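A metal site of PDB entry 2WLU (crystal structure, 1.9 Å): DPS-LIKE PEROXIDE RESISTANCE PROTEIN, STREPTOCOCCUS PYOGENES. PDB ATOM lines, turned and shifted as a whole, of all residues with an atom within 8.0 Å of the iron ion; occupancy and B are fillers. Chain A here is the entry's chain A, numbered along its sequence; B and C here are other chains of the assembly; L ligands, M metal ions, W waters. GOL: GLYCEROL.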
ATOM      1  N   ASN A  73      25.128 -19.837  31.082  1.00  0.00           N
ATOM      2  CA  ASN A  73      25.720 -19.891  29.745  1.00  0.00           C
ATOM      3  C   ASN A  73      26.474 -21.202  29.487  1.00  0.00           C
ATOM      4  O   ASN A  73      26.485 -21.699  28.356  1.00  0.00           O
ATOM      5  CB  ASN A  73      26.611 -18.672  29.508  1.00  0.00           C
ATOM      6  CG  ASN A  73      25.824 -17.465  29.075  1.00  0.00           C
ATOM      7  OD1 ASN A  73      24.851 -17.580  28.309  1.00  0.00           O
ATOM      8  ND2 ASN A  73      26.220 -16.292  29.556  1.00  0.00           N
ATOM      9  N   ALA A  74      27.079 -21.763  30.529  1.00  0.00           N
ATOM     10  CA  ALA A  74      27.693 -23.096  30.428  1.00  0.00           C
ATOM     11  C   ALA A  74      26.621 -24.173  30.158  1.00  0.00           C
ATOM     12  O   ALA A  74      26.817 -25.023  29.289  1.00  0.00           O
ATOM     13  CB  ALA A  74      28.522 -23.448  31.666  1.00  0.00           C
ATOM     14  N   LEU A  76      23.762 -23.585  28.716  1.00  0.00           N
ATOM     15  CA  LEU A  76      23.265 -23.299  27.373  1.00  0.00           C
ATOM     16  C   LEU A  76      24.129 -23.986  26.315  1.00  0.00           C
ATOM     17  O   LEU A  76      23.622 -24.649  25.415  1.00  0.00           O
ATOM     18  CB  LEU A  76      23.233 -21.793  27.093  1.00  0.00           C
ATOM     19  CG  LEU A  76      22.943 -21.330  25.662  1.00  0.00           C
ATOM     20  CD1 LEU A  76      21.514 -21.760  25.221  1.00  0.00           C
ATOM     21  CD2 LEU A  76      23.117 -19.814  25.531  1.00  0.00           C
ATOM     22  N   ASP A  77      25.448 -23.827  26.434  1.00  0.00           N
ATOM     23  CA  ASP A  77      26.356 -24.439  25.468  1.00  0.00           C
ATOM     24  C   ASP A  77      26.236 -25.965  25.487  1.00  0.00           C
ATOM     25  O   ASP A  77      26.171 -26.600  24.430  1.00  0.00           O
ATOM     26  CB  ASP A  77      27.796 -23.960  25.684  1.00  0.00           C
ATOM     27  CG  ASP A  77      28.682 -24.309  24.514  1.00  0.00           C
ATOM     28  OD1 ASP A  77      28.561 -23.666  23.448  1.00  0.00           O
ATOM     29  OD2 ASP A  77      29.495 -25.240  24.652  1.00  0.00           O
ATOM     30  N   GLU A  78      26.185 -26.564  26.671  1.00  0.00           N
ATOM     31  CA  GLU A  78      26.091 -28.018  26.768  1.00  0.00           C
ATOM     32  C   GLU A  78      24.756 -28.552  26.219  1.00  0.00           C
ATOM     33  O   GLU A  78      24.740 -29.539  25.493  1.00  0.00           O
ATOM     34  CB  GLU A  78      26.290 -28.496  28.211  1.00  0.00           C
ATOM     35  CG  GLU A  78      26.377 -30.011  28.329  1.00  0.00           C
ATOM     36  CD  GLU A  78      26.748 -30.482  29.730  1.00  0.00           C
ATOM     37  OE1 GLU A  78      27.044 -29.632  30.602  1.00  0.00           O
ATOM     38  OE2 GLU A  78      26.757 -31.712  29.954  1.00  0.00           O
ATOM     39  N   SER A  80      22.644 -27.028  24.023  1.00  0.00           N
ATOM     40  CA  SER A  80      22.570 -26.802  22.583  1.00  0.00           C
ATOM     41  C   SER A  80      23.390 -27.848  21.831  1.00  0.00           C
ATOM     42  O   SER A  80      22.924 -28.452  20.859  1.00  0.00           O
ATOM     43  CB  SER A  80      23.021 -25.381  22.233  1.00  0.00           C
ATOM     44  OG  SER A  80      23.002 -25.167  20.836  1.00  0.00           O
ATOM     45  N   GLU A  81      24.636 -28.062  22.284  1.00  0.00           N
ATOM     46  CA  GLU A  81      25.497 -29.027  21.611  1.00  0.00           C
ATOM     47  C   GLU A  81      25.021 -30.479  21.763  1.00  0.00           C
ATOM     48  O   GLU A  81      25.229 -31.293  20.867  1.00  0.00           O
ATOM     49  CB  GLU A  81      26.958 -28.837  22.017  1.00  0.00           C
ATOM     50  CG  GLU A  81      27.457 -27.465  21.518  1.00  0.00           C
ATOM     51  CD  GLU A  81      28.842 -27.105  21.987  1.00  0.00           C
ATOM     52  OE1 GLU A  81      29.490 -27.900  22.719  1.00  0.00           O
ATOM     53  OE2 GLU A  81      29.291 -26.004  21.603  1.00  0.00           O
ATOM     54  N   ILE A  84      22.361 -30.720  19.039  1.00  0.00           N
ATOM     55  CA  ILE A  84      23.039 -30.913  17.751  1.00  0.00           C
ATOM     56  C   ILE A  84      23.501 -32.369  17.608  1.00  0.00           C
ATOM     57  O   ILE A  84      23.223 -33.033  16.595  1.00  0.00           O
ATOM     58  CB  ILE A  84      24.299 -30.013  17.613  1.00  0.00           C
ATOM     59  CG1 ILE A  84      23.950 -28.525  17.754  1.00  0.00           C
ATOM     60  CG2 ILE A  84      25.004 -30.255  16.266  1.00  0.00           C
ATOM     61  CD1 ILE A  84      25.178 -27.638  17.950  1.00  0.00           C
ATOM     62  N   HIS B  47      27.494 -17.087  18.087  1.00  0.00           N
ATOM     63  CA  HIS B  47      27.106 -18.369  18.689  1.00  0.00           C
ATOM     64  C   HIS B  47      26.458 -19.303  17.666  1.00  0.00           C
ATOM     65  O   HIS B  47      26.673 -20.515  17.695  1.00  0.00           O
ATOM     66  CB  HIS B  47      26.147 -18.146  19.865  1.00  0.00           C
ATOM     67  CG  HIS B  47      26.553 -18.862  21.127  1.00  0.00           C
ATOM     68  ND1 HIS B  47      25.793 -18.851  22.271  1.00  0.00           N
ATOM     69  CD2 HIS B  47      27.655 -19.606  21.414  1.00  0.00           C
ATOM     70  CE1 HIS B  47      26.396 -19.553  23.215  1.00  0.00           C
ATOM     71  NE2 HIS B  47      27.525 -20.018  22.720  1.00  0.00           N
ATOM     72  N   HIS B  50      29.280 -20.885  15.780  1.00  0.00           N
ATOM     73  CA  HIS B  50      29.850 -21.886  16.694  1.00  0.00           C
ATOM     74  C   HIS B  50      29.066 -23.211  16.610  1.00  0.00           C
ATOM     75  O   HIS B  50      29.658 -24.285  16.510  1.00  0.00           O
ATOM     76  CB  HIS B  50      29.833 -21.285  18.105  1.00  0.00           C
ATOM     77  CG  HIS B  50      30.438 -22.157  19.183  1.00  0.00           C
ATOM     78  ND1 HIS B  50      31.796 -22.375  19.291  1.00  0.00           N
ATOM     79  CD2 HIS B  50      29.866 -22.782  20.242  1.00  0.00           C
ATOM     80  CE1 HIS B  50      32.029 -23.128  20.348  1.00  0.00           C
ATOM     81  NE2 HIS B  50      30.876 -23.392  20.950  1.00  0.00           N
ATOM     82  N   TRP B  51      27.739 -23.123  16.622  1.00  0.00           N
ATOM     83  CA  TRP B  51      26.926 -24.340  16.679  1.00  0.00           C
ATOM     84  C   TRP B  51      26.670 -25.006  15.319  1.00  0.00           C
ATOM     85  O   TRP B  51      26.742 -26.225  15.214  1.00  0.00           O
ATOM     86  CB  TRP B  51      25.593 -24.060  17.389  1.00  0.00           C
ATOM     87  CG  TRP B  51      25.740 -23.781  18.871  1.00  0.00           C
ATOM     88  CD1 TRP B  51      26.686 -24.274  19.725  1.00  0.00           C
ATOM     89  CD2 TRP B  51      24.874 -22.956  19.662  1.00  0.00           C
ATOM     90  NE1 TRP B  51      26.482 -23.795  21.007  1.00  0.00           N
ATOM     91  CE2 TRP B  51      25.382 -22.976  20.991  1.00  0.00           C
ATOM     92  CE3 TRP B  51      23.728 -22.201  19.378  1.00  0.00           C
ATOM     93  CZ2 TRP B  51      24.756 -22.277  22.039  1.00  0.00           C
ATOM     94  CZ3 TRP B  51      23.116 -21.492  20.427  1.00  0.00           C
ATOM     95  CH2 TRP B  51      23.637 -21.538  21.739  1.00  0.00           C
ATOM     96  N   HIS B  62      35.632 -23.389  15.259  1.00  0.00           N
ATOM     97  CA  HIS B  62      34.683 -23.565  16.357  1.00  0.00           C
ATOM     98  C   HIS B  62      35.186 -22.923  17.668  1.00  0.00           C
ATOM     99  O   HIS B  62      34.462 -22.111  18.260  1.00  0.00           O
ATOM    100  CB  HIS B  62      34.366 -25.057  16.512  1.00  0.00           C
ATOM    101  CG  HIS B  62      33.427 -25.393  17.638  1.00  0.00           C
ATOM    102  ND1 HIS B  62      32.063 -25.224  17.539  1.00  0.00           N
ATOM    103  CD2 HIS B  62      33.662 -25.971  18.836  1.00  0.00           C
ATOM    104  CE1 HIS B  62      31.500 -25.658  18.663  1.00  0.00           C
ATOM    105  NE2 HIS B  62      32.442 -26.109  19.458  1.00  0.00           N
ATOM    106  N   PRO B  63      36.410 -23.260  18.121  1.00  0.00           N
ATOM    107  CA  PRO B  63      36.878 -22.573  19.344  1.00  0.00           C
ATOM    108  C   PRO B  63      37.202 -21.083  19.127  1.00  0.00           C
ATOM    109  O   PRO B  63      37.075 -20.315  20.064  1.00  0.00           O
ATOM    110  CB  PRO B  63      38.144 -23.355  19.741  1.00  0.00           C
ATOM    111  CG  PRO B  63      38.585 -24.055  18.485  1.00  0.00           C
ATOM    112  CD  PRO B  63      37.292 -24.384  17.756  1.00  0.00           C
ATOM    113  N   ASP B  66      34.324 -19.018  20.166  1.00  0.00           N
ATOM    114  CA  ASP B  66      34.257 -18.757  21.606  1.00  0.00           C
ATOM    115  C   ASP B  66      35.120 -17.576  22.053  1.00  0.00           C
ATOM    116  O   ASP B  66      34.707 -16.828  22.952  1.00  0.00           O
ATOM    117  CB  ASP B  66      34.560 -20.001  22.434  1.00  0.00           C
ATOM    118  CG  ASP B  66      33.334 -20.869  22.660  1.00  0.00           C
ATOM    119  OD1 ASP B  66      33.527 -22.044  23.054  1.00  0.00           O
ATOM    120  OD2 ASP B  66      32.184 -20.403  22.434  1.00  0.00           O
ATOM    121  N   LEU B  69      33.178 -14.575  20.914  1.00  0.00           N
ATOM    122  CA  LEU B  69      32.017 -14.436  21.803  1.00  0.00           C
ATOM    123  C   LEU B  69      32.406 -13.820  23.145  1.00  0.00           C
ATOM    124  O   LEU B  69      31.735 -12.884  23.627  1.00  0.00           O
ATOM    125  CB  LEU B  69      31.363 -15.803  22.013  1.00  0.00           C
ATOM    126  CG  LEU B  69      30.087 -15.846  22.867  1.00  0.00           C
ATOM    127  CD1 LEU B  69      28.905 -15.233  22.116  1.00  0.00           C
ATOM    128  CD2 LEU B  69      29.772 -17.290  23.279  1.00  0.00           C
ATOM    129  N   LYS C 160      29.701 -36.713  21.470  1.00  0.00           N
ATOM    130  CA  LYS C 160      30.229 -35.361  21.250  1.00  0.00           C
ATOM    131  C   LYS C 160      31.408 -35.388  20.273  1.00  0.00           C
ATOM    132  O   LYS C 160      31.498 -34.554  19.373  1.00  0.00           O
ATOM    133  CB  LYS C 160      30.673 -34.748  22.574  1.00  0.00           C
ATOM    134  CG  LYS C 160      31.255 -33.330  22.421  1.00  0.00           C
ATOM    135  CD  LYS C 160      31.443 -32.680  23.794  1.00  0.00           C
ATOM    136  CE  LYS C 160      31.936 -31.251  23.642  1.00  0.00           C
ATOM    137  NZ  LYS C 160      32.054 -30.592  25.001  1.00  0.00           N
ATOM    138  N   TRP C 163      30.073 -35.859  16.744  1.00  0.00           N
ATOM    139  CA  TRP C 163      29.563 -34.575  16.216  1.00  0.00           C
ATOM    140  C   TRP C 163      30.702 -33.694  15.685  1.00  0.00           C
ATOM    141  O   TRP C 163      30.635 -33.195  14.567  1.00  0.00           O
ATOM    142  CB  TRP C 163      28.693 -33.821  17.253  1.00  0.00           C
ATOM    143  CG  TRP C 163      28.686 -32.305  17.020  1.00  0.00           C
ATOM    144  CD1 TRP C 163      28.281 -31.653  15.881  1.00  0.00           C
ATOM    145  CD2 TRP C 163      29.108 -31.291  17.940  1.00  0.00           C
ATOM    146  NE1 TRP C 163      28.442 -30.295  16.036  1.00  0.00           N
ATOM    147  CE2 TRP C 163      28.946 -30.043  17.293  1.00  0.00           C
ATOM    148  CE3 TRP C 163      29.599 -31.315  19.255  1.00  0.00           C
ATOM    149  CZ2 TRP C 163      29.261 -28.827  17.912  1.00  0.00           C
ATOM    150  CZ3 TRP C 163      29.928 -30.107  19.867  1.00  0.00           C
ATOM    151  CH2 TRP C 163      29.761 -28.879  19.194  1.00  0.00           C
ATOM    152  N   MET C 164      31.744 -33.520  16.485  1.00  0.00           N
ATOM    153  CA  MET C 164      32.847 -32.625  16.104  1.00  0.00           C
ATOM    154  C   MET C 164      33.692 -33.130  14.932  1.00  0.00           C
ATOM    155  O   MET C 164      34.053 -32.348  14.036  1.00  0.00           O
ATOM    156  CB  MET C 164      33.736 -32.302  17.320  1.00  0.00           C
ATOM    157  CG  MET C 164      32.950 -31.566  18.388  1.00  0.00           C
ATOM    158  SD  MET C 164      33.921 -31.017  19.795  1.00  0.00           S
ATOM    159  CE  MET C 164      34.801 -29.628  19.096  1.00  0.00           C
HETATM  160  C1  GOL L   1      32.709 -28.121  23.108  1.00  0.00           C
HETATM  161  O1  GOL L   1      31.817 -27.995  24.187  1.00  0.00           O
HETATM  162  C2  GOL L   1      33.814 -27.096  23.282  1.00  0.00           C
HETATM  163  O2  GOL L   1      34.993 -27.628  22.695  1.00  0.00           O
HETATM  164  C3  GOL L   1      33.418 -25.819  22.566  1.00  0.00           C
HETATM  165  O3  GOL L   1      32.098 -25.908  22.070  1.00  0.00           O
HETATM  166 FE    FE M   1      30.479 -24.733  22.649  1.00  0.00          FE
HETATM  167  O   HOH W   1      31.748 -23.567  23.938  1.00  0.00           O
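ND1 of His 62 of chain B lies within hydrogen-bond range of O of His 50 of chain B (2.8 Å).
The side-chain carboxylate (OD1) of Asp 77 lies close to the indole nitrogen (NE1) of Trp 51 of chain B (3.2 Å).
The iron ion is bound by OE2 of Glu 81 (2.0 Å), O3 of the ligand (2.1 Å), water W1 (2.2 Å), NE2 of His 50 of chain B (2.2 Å), OD2 of Asp 77 (2.3 Å) and OD1 of Asp 77 (2.3 Å).
His 62 of chain B touches the iron ion.
Within 4 Å of the iron ion: Asp 77, Glu 81, His 50 of chain B and His 62 of chain B.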
